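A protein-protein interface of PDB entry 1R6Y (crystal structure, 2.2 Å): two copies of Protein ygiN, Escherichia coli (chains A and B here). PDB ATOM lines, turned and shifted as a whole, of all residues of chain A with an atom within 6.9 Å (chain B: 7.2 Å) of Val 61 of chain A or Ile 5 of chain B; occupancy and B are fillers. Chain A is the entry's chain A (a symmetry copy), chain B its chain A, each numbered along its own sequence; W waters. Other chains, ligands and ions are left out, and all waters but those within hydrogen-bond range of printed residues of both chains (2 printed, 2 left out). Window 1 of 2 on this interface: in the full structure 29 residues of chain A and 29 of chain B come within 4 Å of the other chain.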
ATOM      1  N   ILE A   5     -17.709  -2.149  24.907  1.00  0.00           N
ATOM      2  CA  ILE A   5     -17.836  -1.576  23.551  1.00  0.00           C
ATOM      3  C   ILE A   5     -18.250  -0.112  23.752  1.00  0.00           C
ATOM      4  O   ILE A   5     -19.347   0.152  24.297  1.00  0.00           O
ATOM      5  CB  ILE A   5     -18.899  -2.299  22.762  1.00  0.00           C
ATOM      6  CG1 ILE A   5     -18.499  -3.736  22.469  1.00  0.00           C
ATOM      7  CG2 ILE A   5     -19.098  -1.554  21.429  1.00  0.00           C
ATOM      8  CD1 ILE A   5     -19.628  -4.394  21.815  1.00  0.00           C
ATOM      9  N   ALA A   6     -17.370   0.829  23.419  1.00  0.00           N
ATOM     10  CA  ALA A   6     -17.674   2.249  23.678  1.00  0.00           C
ATOM     11  C   ALA A   6     -17.784   2.897  22.349  1.00  0.00           C
ATOM     12  O   ALA A   6     -16.816   2.928  21.606  1.00  0.00           O
ATOM     13  CB  ALA A   6     -16.562   2.918  24.452  1.00  0.00           C
ATOM     14  N   GLU A   7     -18.920   3.476  22.053  1.00  0.00           N
ATOM     15  CA  GLU A   7     -19.034   4.189  20.790  1.00  0.00           C
ATOM     16  C   GLU A   7     -18.887   5.650  20.983  1.00  0.00           C
ATOM     17  O   GLU A   7     -19.558   6.218  21.824  1.00  0.00           O
ATOM     18  CB  GLU A   7     -20.370   3.932  20.162  1.00  0.00           C
ATOM     19  CG  GLU A   7     -20.532   4.661  18.831  1.00  0.00           C
ATOM     20  CD  GLU A   7     -21.611   4.039  17.924  1.00  0.00           C
ATOM     21  OE1 GLU A   7     -22.382   3.149  18.385  1.00  0.00           O
ATOM     22  OE2 GLU A   7     -21.619   4.376  16.723  1.00  0.00           O
ATOM     23  N   ILE A   8     -17.955   6.204  20.222  1.00  0.00           N
ATOM     24  CA  ILE A   8     -17.578   7.536  20.356  1.00  0.00           C
ATOM     25  C   ILE A   8     -18.074   8.254  19.104  1.00  0.00           C
ATOM     26  O   ILE A   8     -17.689   7.896  17.987  1.00  0.00           O
ATOM     27  CB  ILE A   8     -16.102   7.687  20.391  1.00  0.00           C
ATOM     28  CG1 ILE A   8     -15.506   7.074  21.710  1.00  0.00           C
ATOM     29  CG2 ILE A   8     -15.747   9.160  20.331  1.00  0.00           C
ATOM     30  CD1 ILE A   8     -13.984   6.971  21.521  1.00  0.00           C
ATOM     31  N   ALA A  41      -9.055  -1.621  21.090  1.00  0.00           N
ATOM     32  CA  ALA A  41      -8.874  -1.350  19.645  1.00  0.00           C
ATOM     33  C   ALA A  41      -9.941  -0.333  19.138  1.00  0.00           C
ATOM     34  O   ALA A  41     -11.133  -0.611  19.290  1.00  0.00           O
ATOM     35  CB  ALA A  41      -9.018  -2.667  18.946  1.00  0.00           C
ATOM     36  N   PRO A  42      -9.521   0.787  18.564  1.00  0.00           N
ATOM     37  CA  PRO A  42     -10.449   1.742  17.943  1.00  0.00           C
ATOM     38  C   PRO A  42     -10.772   1.342  16.537  1.00  0.00           C
ATOM     39  O   PRO A  42      -9.874   1.178  15.733  1.00  0.00           O
ATOM     40  CB  PRO A  42      -9.689   3.081  17.956  1.00  0.00           C
ATOM     41  CG  PRO A  42      -8.224   2.682  18.001  1.00  0.00           C
ATOM     42  CD  PRO A  42      -8.122   1.285  18.550  1.00  0.00           C
ATOM     43  N   MET A  43     -12.025   1.079  16.270  1.00  0.00           N
ATOM     44  CA  MET A  43     -12.443   0.480  14.997  1.00  0.00           C
ATOM     45  C   MET A  43     -13.274   1.551  14.299  1.00  0.00           C
ATOM     46  O   MET A  43     -13.897   2.380  14.949  1.00  0.00           O
ATOM     47  CB  MET A  43     -13.301  -0.760  15.264  1.00  0.00           C
ATOM     48  CG  MET A  43     -12.636  -1.816  16.207  1.00  0.00           C
ATOM     49  SD  MET A  43     -11.083  -2.410  15.461  1.00  0.00           S
ATOM     50  CE  MET A  43     -10.853  -3.686  16.566  1.00  0.00           C
ATOM     51  N   VAL A  44     -13.215   1.605  13.005  1.00  0.00           N
ATOM     52  CA  VAL A  44     -14.139   2.423  12.183  1.00  0.00           C
ATOM     53  C   VAL A  44     -14.879   1.546  11.116  1.00  0.00           C
ATOM     54  O   VAL A  44     -14.403   0.485  10.756  1.00  0.00           O
ATOM     55  CB  VAL A  44     -13.387   3.516  11.468  1.00  0.00           C
ATOM     56  CG1 VAL A  44     -12.809   4.472  12.413  1.00  0.00           C
ATOM     57  CG2 VAL A  44     -12.313   2.974  10.557  1.00  0.00           C
ATOM     58  N   ASP A  45     -16.040   2.005  10.614  1.00  0.00           N
ATOM     59  CA  ASP A  45     -16.715   1.267   9.550  1.00  0.00           C
ATOM     60  C   ASP A  45     -15.804   1.005   8.358  1.00  0.00           C
ATOM     61  O   ASP A  45     -14.929   1.822   7.990  1.00  0.00           O
ATOM     62  CB  ASP A  45     -18.010   1.902   9.091  1.00  0.00           C
ATOM     63  CG  ASP A  45     -18.989   2.055  10.173  1.00  0.00           C
ATOM     64  OD1 ASP A  45     -19.343   1.038  10.805  1.00  0.00           O
ATOM     65  OD2 ASP A  45     -19.383   3.222  10.608  1.00  0.00           O
ATOM     66  N   SER A  59     -18.233   8.095  13.727  1.00  0.00           N
ATOM     67  CA  SER A  59     -18.263   7.188  14.861  1.00  0.00           C
ATOM     68  C   SER A  59     -16.911   6.369  14.958  1.00  0.00           C
ATOM     69  O   SER A  59     -16.359   5.969  13.955  1.00  0.00           O
ATOM     70  CB  SER A  59     -19.517   6.302  14.803  1.00  0.00           C
ATOM     71  OG  SER A  59     -19.178   4.982  14.733  1.00  0.00           O
ATOM     72  N   ILE A  60     -16.418   6.160  16.164  1.00  0.00           N
ATOM     73  CA  ILE A  60     -15.311   5.222  16.401  1.00  0.00           C
ATOM     74  C   ILE A  60     -15.849   4.264  17.376  1.00  0.00           C
ATOM     75  O   ILE A  60     -16.477   4.694  18.377  1.00  0.00           O
ATOM     76  CB  ILE A  60     -14.166   5.962  17.023  1.00  0.00           C
ATOM     77  CG1 ILE A  60     -13.532   6.861  15.919  1.00  0.00           C
ATOM     78  CG2 ILE A  60     -13.112   5.016  17.676  1.00  0.00           C
ATOM     79  CD1 ILE A  60     -12.686   7.889  16.477  1.00  0.00           C
ATOM     80  N   VAL A  61     -15.630   2.979  17.140  1.00  0.00           N
ATOM     81  CA  VAL A  61     -16.128   2.003  18.053  1.00  0.00           C
ATOM     82  C   VAL A  61     -14.930   1.359  18.756  1.00  0.00           C
ATOM     83  O   VAL A  61     -14.082   0.753  18.107  1.00  0.00           O
ATOM     84  CB  VAL A  61     -16.926   0.950  17.339  1.00  0.00           C
ATOM     85  CG1 VAL A  61     -17.441  -0.117  18.312  1.00  0.00           C
ATOM     86  CG2 VAL A  61     -18.171   1.547  16.533  1.00  0.00           C
ATOM     87  N   MET A  62     -14.881   1.481  20.088  1.00  0.00           N
ATOM     88  CA  MET A  62     -13.774   0.898  20.871  1.00  0.00           C
ATOM     89  C   MET A  62     -14.192  -0.469  21.312  1.00  0.00           C
ATOM     90  O   MET A  62     -15.259  -0.644  21.828  1.00  0.00           O
ATOM     91  CB  MET A  62     -13.411   1.707  22.092  1.00  0.00           C
ATOM     92  CG  MET A  62     -13.023   3.172  21.826  1.00  0.00           C
ATOM     93  SD  MET A  62     -11.634   3.483  20.850  1.00  0.00           S
ATOM     94  CE  MET A  62     -10.575   2.498  21.911  1.00  0.00           C
ATOM     95  N   ILE A  63     -13.378  -1.466  20.982  1.00  0.00           N
ATOM     96  CA  ILE A  63     -13.602  -2.786  21.536  1.00  0.00           C
ATOM     97  C   ILE A  63     -12.484  -3.097  22.500  1.00  0.00           C
ATOM     98  O   ILE A  63     -11.323  -3.068  22.140  1.00  0.00           O
ATOM     99  CB  ILE A  63     -13.690  -3.854  20.368  1.00  0.00           C
ATOM    100  CG1 ILE A  63     -14.733  -3.411  19.371  1.00  0.00           C
ATOM    101  CG2 ILE A  63     -13.946  -5.268  20.916  1.00  0.00           C
ATOM    102  CD1 ILE A  63     -14.764  -4.270  18.131  1.00  0.00           C
ATOM    103  N   THR B   3     -14.124  -7.080  11.640  1.00  0.00           N
ATOM    104  CA  THR B   3     -14.872  -7.297  12.888  1.00  0.00           C
ATOM    105  C   THR B   3     -16.319  -6.873  12.699  1.00  0.00           C
ATOM    106  O   THR B   3     -16.600  -5.811  12.136  1.00  0.00           O
ATOM    107  CB  THR B   3     -14.259  -6.467  14.039  1.00  0.00           C
ATOM    108  OG1 THR B   3     -12.892  -6.819  14.193  1.00  0.00           O
ATOM    109  CG2 THR B   3     -15.002  -6.687  15.410  1.00  0.00           C
ATOM    110  N   VAL B   4     -17.217  -7.736  13.089  1.00  0.00           N
ATOM    111  CA  VAL B   4     -18.640  -7.527  12.912  1.00  0.00           C
ATOM    112  C   VAL B   4     -19.166  -7.362  14.274  1.00  0.00           C
ATOM    113  O   VAL B   4     -18.882  -8.168  15.191  1.00  0.00           O
ATOM    114  CB  VAL B   4     -19.333  -8.694  12.287  1.00  0.00           C
ATOM    115  CG1 VAL B   4     -20.883  -8.546  12.396  1.00  0.00           C
ATOM    116  CG2 VAL B   4     -18.921  -8.732  10.839  1.00  0.00           C
ATOM    117  N   ILE B   5     -19.871  -6.257  14.486  1.00  0.00           N
ATOM    118  CA  ILE B   5     -20.634  -6.113  15.743  1.00  0.00           C
ATOM    119  C   ILE B   5     -22.110  -6.050  15.333  1.00  0.00           C
ATOM    120  O   ILE B   5     -22.517  -5.102  14.621  1.00  0.00           O
ATOM    121  CB  ILE B   5     -20.252  -4.840  16.457  1.00  0.00           C
ATOM    122  CG1 ILE B   5     -18.816  -4.885  16.952  1.00  0.00           C
ATOM    123  CG2 ILE B   5     -21.192  -4.666  17.663  1.00  0.00           C
ATOM    124  CD1 ILE B   5     -18.492  -3.576  17.518  1.00  0.00           C
ATOM    125  N   ALA B   6     -22.890  -7.073  15.677  1.00  0.00           N
ATOM    126  CA  ALA B   6     -24.295  -7.114  15.229  1.00  0.00           C
ATOM    127  C   ALA B   6     -25.122  -7.006  16.454  1.00  0.00           C
ATOM    128  O   ALA B   6     -25.055  -7.872  17.312  1.00  0.00           O
ATOM    129  CB  ALA B   6     -24.616  -8.421  14.543  1.00  0.00           C
ATOM    130  N   GLU B   7     -25.953  -5.997  16.533  1.00  0.00           N
ATOM    131  CA  GLU B   7     -26.836  -5.906  17.685  1.00  0.00           C
ATOM    132  C   GLU B   7     -28.199  -6.386  17.358  1.00  0.00           C
ATOM    133  O   GLU B   7     -28.773  -5.949  16.379  1.00  0.00           O
ATOM    134  CB  GLU B   7     -26.941  -4.487  18.154  1.00  0.00           C
ATOM    135  CG  GLU B   7     -27.858  -4.345  19.366  1.00  0.00           C
ATOM    136  CD  GLU B   7     -27.593  -3.065  20.182  1.00  0.00           C
ATOM    137  OE1 GLU B   7     -26.824  -2.173  19.721  1.00  0.00           O
ATOM    138  OE2 GLU B   7     -28.082  -3.002  21.329  1.00  0.00           O
ATOM    139  N   VAL B  61     -25.459  -8.555  21.865  1.00  0.00           N
ATOM    140  CA  VAL B  61     -24.491  -7.957  21.003  1.00  0.00           C
ATOM    141  C   VAL B  61     -23.530  -9.055  20.539  1.00  0.00           C
ATOM    142  O   VAL B  61     -22.857  -9.677  21.357  1.00  0.00           O
ATOM    143  CB  VAL B  61     -23.726  -6.878  21.714  1.00  0.00           C
ATOM    144  CG1 VAL B  61     -22.666  -6.251  20.801  1.00  0.00           C
ATOM    145  CG2 VAL B  61     -24.664  -5.713  22.278  1.00  0.00           C
ATOM    146  N   MET B  62     -23.461  -9.272  19.220  1.00  0.00           N
ATOM    147  CA  MET B  62     -22.568 -10.304  18.658  1.00  0.00           C
ATOM    148  C   MET B  62     -21.267  -9.648  18.315  1.00  0.00           C
ATOM    149  O   MET B  62     -21.245  -8.631  17.683  1.00  0.00           O
ATOM    150  CB  MET B  62     -23.117 -10.962  17.417  1.00  0.00           C
ATOM    151  CG  MET B  62     -24.495 -11.628  17.573  1.00  0.00           C
ATOM    152  SD  MET B  62     -24.645 -12.939  18.687  1.00  0.00           S
ATOM    153  CE  MET B  62     -23.335 -13.866  17.888  1.00  0.00           C
ATOM    154  N   ILE B  63     -20.179 -10.187  18.855  1.00  0.00           N
ATOM    155  CA  ILE B  63     -18.871  -9.742  18.421  1.00  0.00           C
ATOM    156  C   ILE B  63     -18.214 -10.863  17.654  1.00  0.00           C
ATOM    157  O   ILE B  63     -18.055 -11.956  18.159  1.00  0.00           O
ATOM    158  CB  ILE B  63     -18.007  -9.300  19.675  1.00  0.00           C
ATOM    159  CG1 ILE B  63     -18.781  -8.277  20.472  1.00  0.00           C
ATOM    160  CG2 ILE B  63     -16.614  -8.803  19.253  1.00  0.00           C
ATOM    161  CD1 ILE B  63     -18.119  -7.927  21.781  1.00  0.00           C
ATOM    162  N   GLU B  64     -17.831 -10.582  16.408  1.00  0.00           N
ATOM    163  CA  GLU B  64     -17.421 -11.597  15.481  1.00  0.00           C
ATOM    164  C   GLU B  64     -16.181 -11.142  14.754  1.00  0.00           C
ATOM    165  O   GLU B  64     -15.938  -9.952  14.587  1.00  0.00           O
ATOM    166  CB  GLU B  64     -18.520 -11.852  14.405  1.00  0.00           C
ATOM    167  CG  GLU B  64     -19.913 -11.978  15.000  1.00  0.00           C
ATOM    168  CD  GLU B  64     -21.021 -12.140  13.951  1.00  0.00           C
ATOM    169  OE1 GLU B  64     -20.707 -12.518  12.826  1.00  0.00           O
ATOM    170  OE2 GLU B  64     -22.221 -11.915  14.297  1.00  0.00           O
ATOM    171  N   MET B  95     -31.927  -6.360  13.649  1.00  0.00           N
ATOM    172  CA  MET B  95     -30.468  -6.601  13.806  1.00  0.00           C
ATOM    173  C   MET B  95     -29.710  -5.520  13.061  1.00  0.00           C
ATOM    174  O   MET B  95     -29.991  -5.320  11.896  1.00  0.00           O
ATOM    175  CB  MET B  95     -30.116  -7.933  13.217  1.00  0.00           C
ATOM    176  CG  MET B  95     -28.693  -8.430  13.387  1.00  0.00           C
ATOM    177  SD  MET B  95     -28.630 -10.279  13.152  1.00  0.00           S
ATOM    178  CE  MET B  95     -29.421 -10.379  11.794  1.00  0.00           C
ATOM    179  N   ASN B  96     -28.808  -4.826  13.736  1.00  0.00           N
ATOM    180  CA  ASN B  96     -27.961  -3.724  13.164  1.00  0.00           C
ATOM    181  C   ASN B  96     -26.532  -4.292  13.043  1.00  0.00           C
ATOM    182  O   ASN B  96     -25.918  -4.544  14.100  1.00  0.00           O
ATOM    183  CB  ASN B  96     -28.002  -2.549  14.160  1.00  0.00           C
ATOM    184  CG  ASN B  96     -27.182  -1.232  13.695  1.00  0.00           C
ATOM    185  OD1 ASN B  96     -26.123  -0.889  14.280  1.00  0.00           O
ATOM    186  ND2 ASN B  96     -27.698  -0.512  12.720  1.00  0.00           N
ATOM    187  N   ILE B  97     -26.058  -4.528  11.808  1.00  0.00           N
ATOM    188  CA  ILE B  97     -24.793  -5.085  11.513  1.00  0.00           C
ATOM    189  C   ILE B  97     -23.784  -4.031  11.150  1.00  0.00           C
ATOM    190  O   ILE B  97     -23.945  -3.366  10.149  1.00  0.00           O
ATOM    191  CB  ILE B  97     -24.946  -6.030  10.450  1.00  0.00           C
ATOM    192  CG1 ILE B  97     -25.902  -7.170  10.874  1.00  0.00           C
ATOM    193  CG2 ILE B  97     -23.625  -6.644  10.083  1.00  0.00           C
ATOM    194  CD1 ILE B  97     -26.192  -8.164   9.757  1.00  0.00           C
ATOM    195  N   ARG B  98     -22.804  -3.772  12.042  1.00  0.00           N
ATOM    196  CA  ARG B  98     -21.586  -3.118  11.638  1.00  0.00           C
ATOM    197  C   ARG B  98     -20.449  -4.042  11.295  1.00  0.00           C
ATOM    198  O   ARG B  98     -20.146  -4.958  12.058  1.00  0.00           O
ATOM    199  CB  ARG B  98     -21.075  -2.160  12.705  1.00  0.00           C
ATOM    200  CG  ARG B  98     -22.228  -1.367  13.260  1.00  0.00           C
ATOM    201  CD  ARG B  98     -22.129   0.004  13.402  1.00  0.00           C
ATOM    202  NE  ARG B  98     -21.052   0.873  12.860  1.00  0.00           N
ATOM    203  CZ  ARG B  98     -20.666   1.901  13.644  1.00  0.00           C
ATOM    204  NH1 ARG B  98     -21.279   2.062  14.821  1.00  0.00           N
ATOM    205  NH2 ARG B  98     -19.752   2.784  13.273  1.00  0.00           N
ATOM    206  N   ILE B  99     -19.671  -3.549  10.332  1.00  0.00           N
ATOM    207  CA  ILE B  99     -18.554  -4.221   9.801  1.00  0.00           C
ATOM    208  C   ILE B  99     -17.442  -3.200   9.890  1.00  0.00           C
ATOM    209  O   ILE B  99     -17.459  -2.187   9.193  1.00  0.00           O
ATOM    210  CB  ILE B  99     -18.760  -4.598   8.293  1.00  0.00           C
ATOM    211  CG1 ILE B  99     -20.041  -5.370   8.087  1.00  0.00           C
ATOM    212  CG2 ILE B  99     -17.564  -5.550   7.840  1.00  0.00           C
ATOM    213  CD1 ILE B  99     -20.268  -5.865   6.615  1.00  0.00           C
ATOM    214  N   LEU B 100     -16.438  -3.576  10.644  1.00  0.00           N
ATOM    215  CA  LEU B 100     -15.464  -2.609  11.104  1.00  0.00           C
ATOM    216  C   LEU B 100     -14.034  -3.110  10.718  1.00  0.00           C
ATOM    217  O   LEU B 100     -13.833  -4.265  10.593  1.00  0.00           O
ATOM    218  CB  LEU B 100     -15.536  -2.565  12.636  1.00  0.00           C
ATOM    219  CG  LEU B 100     -16.913  -2.166  13.278  1.00  0.00           C
ATOM    220  CD1 LEU B 100     -16.933  -2.395  14.708  1.00  0.00           C
ATOM    221  CD2 LEU B 100     -17.029  -0.684  13.045  1.00  0.00           C
ATOM    222  N   GLN B 101     -13.093  -2.183  10.658  1.00  0.00           N
ATOM    223  CA  GLN B 101     -11.676  -2.499  10.586  1.00  0.00           C
ATOM    224  C   GLN B 101     -10.922  -1.549  11.536  1.00  0.00           C
ATOM    225  O   GLN B 101     -11.503  -0.572  12.030  1.00  0.00           O
ATOM    226  CB  GLN B 101     -11.183  -2.240   9.149  1.00  0.00           C
ATOM    227  CG  GLN B 101     -11.252  -0.813   8.807  1.00  0.00           C
ATOM    228  CD  GLN B 101     -10.983  -0.609   7.371  1.00  0.00           C
ATOM    229  OE1 GLN B 101     -10.489  -1.545   6.702  1.00  0.00           O
ATOM    230  NE2 GLN B 101     -11.269   0.585   6.871  1.00  0.00           N
ATOM    231  N   GLY B 103      -9.028   1.379  13.117  1.00  0.00           N
ATOM    232  CA  GLY B 103      -9.104   2.753  12.648  1.00  0.00           C
ATOM    233  C   GLY B 103      -7.878   3.597  12.940  1.00  0.00           C
ATOM    234  O   GLY B 103      -7.436   4.440  12.148  1.00  0.00           O
HETATM  235  O   HOH W   1     -17.120   4.343  11.767  1.00  0.00           O
HETATM  236  O   HOH W   2     -23.152   0.621  16.613  1.00  0.00           O
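The guanidinium group of Arg 98 of chain B lies within salt-bridge range of the side-chain carboxylate of Glu 7 of chain A, at 3.0 Å.
The backbone NH (N) of Gly 103 of chain B lies within hydrogen-bond range of the backbone carbonyl oxygen (O) of Pro 42 of chain A (2.8 Å).
The backbone carbonyl oxygen (O) of Gln 101 of chain B lies within hydrogen-bond range of the backbone NH (N) of Val 44 of chain A (2.9 Å).
The guanidinium group (NE) of Arg 98 of chain B lies within salt-bridge range of the side-chain carboxylate (OD1) of Asp 45 of chain A, 2.7 Å away.
The side-chain hydroxyl (OG) of Ser 59 of chain A lies within hydrogen-bond range of the guanidinium group (NH2) of Arg 98 of chain B, at 2.7 Å.
Among the printed residues, merely in contact across the chains: Ile 5 of chain A with Val 61 of chain B (3.7 Å), Ile 5 of chain A with Ile 63 of chain B (3.8 Å), Met 43 of chain A with Leu 100 of chain B (3.9 Å), Met 43 of chain A with Gln 101 of chain B (3.3 Å), Val 44 of chain A with Leu 100 of chain B (3.3 Å), Val 44 of chain A with Gly 103 of chain B (3.8 Å), Asp 45 of chain A with Ile 99 of chain B (3.6 Å), Asp 45 of chain A with Leu 100 of chain B (3.7 Å), Val 61 of chain A with Ile 5 of chain B (3.7 Å), Val 61 of chain A with Arg 98 of chain B (3.6 Å), Ile 63 of chain A with Thr 3 of chain B (3.6 Å) and Ile 63 of chain A with Ile 5 of chain B (3.8 Å).
Of the printed residues of chain B, Ile 5 of chain A touches Val 61 (3.7 Å) and Ile 63 (3.8 Å).
Ala 41 of chain A touches none of the printed residues of chain B.
Val 61 of chain A touches two residues of chain B.
Of chain A, only Val 61 and Ile 63 come within 4 Å of Ile 5 of chain B.
Printed residues of chain A within 4 Å of Val 61 of chain B: Ile 5 (3.7 Å).
The nearest printed residue of chain A that does not touch Thr 3 of chain B is Met 43 of chain A (4.4 Å).
Of the 14 printed residues of chain A, 9 touch a printed residue of chain B.
Hydrophobic or aromatic side chains of chain A within 4 Å of the printed part of chain B: Ile 5, Met 43, Val 44, Val 61 and Ile 63.
Of the 17 printed residues of chain B, 9 touch a printed residue of chain A.
Hydrophobic or aromatic side chains of chain B within 4 Å of the printed part of chain A: Ile 5, Val 61, Ile 63 and Leu 100.
Among the printed residues, 17 pairs touch across the chains.
Among the printed residues, Asp or Glu carboxylates within 4 Å of a Lys or Arg side-chain nitrogen of the other chain: Glu 7 of chain A with Arg 98 of chain B (3.0 Å) and Asp 45 of chain A with Arg 98 of chain B (2.7 Å).
Water W1 lies within hydrogen-bond range of the side-chain carboxylate of Asp 45 of chain A (2.8 Å), the backbone carbonyl oxygen of Ser 59 of chain A (2.8 Å) and the guanidinium group of Arg 98 of chain B (3.4 Å).
Water W2 lies within hydrogen-bond range of NH1 of Arg 98 of chain B (3.0 Å) and OE1 of Glu 7 of chain A (3.2 Å).
Ile 5 of chain A touches Val 61 of chain B, and with the chains exchanged Val 61 of chain A touches Ile 5 of chain B.
Ile 5 of chain A touches Ile 63 of chain B, and with the chains exchanged Ile 63 of chain A touches Ile 5 of chain B.
The side-chain hydroxyl (OG) of Ser 59 of chain A lies within hydrogen-bond range of the side-chain carboxylate (OE2) of Glu 7 of chain A, at 3.2 Å.
The backbone carbonyl oxygen (O) of Thr 3 of chain B lies within hydrogen-bond range of the backbone NH (N) of Leu 100 of chain B (2.7 Å).
O of Ile 63 of chain A sits at hydrogen-bond distance from N of Ala 41 of chain A, at 2.9 Å.
The backbone NH (N) of Met 43 of chain A lies within hydrogen-bond range of the backbone carbonyl oxygen (O) of Val 61 of chain A (2.8 Å).
The backbone carbonyl oxygen of Arg 98 of chain B lies within hydrogen-bond range of the backbone NH of Ile 5 of chain B (2.8 Å).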
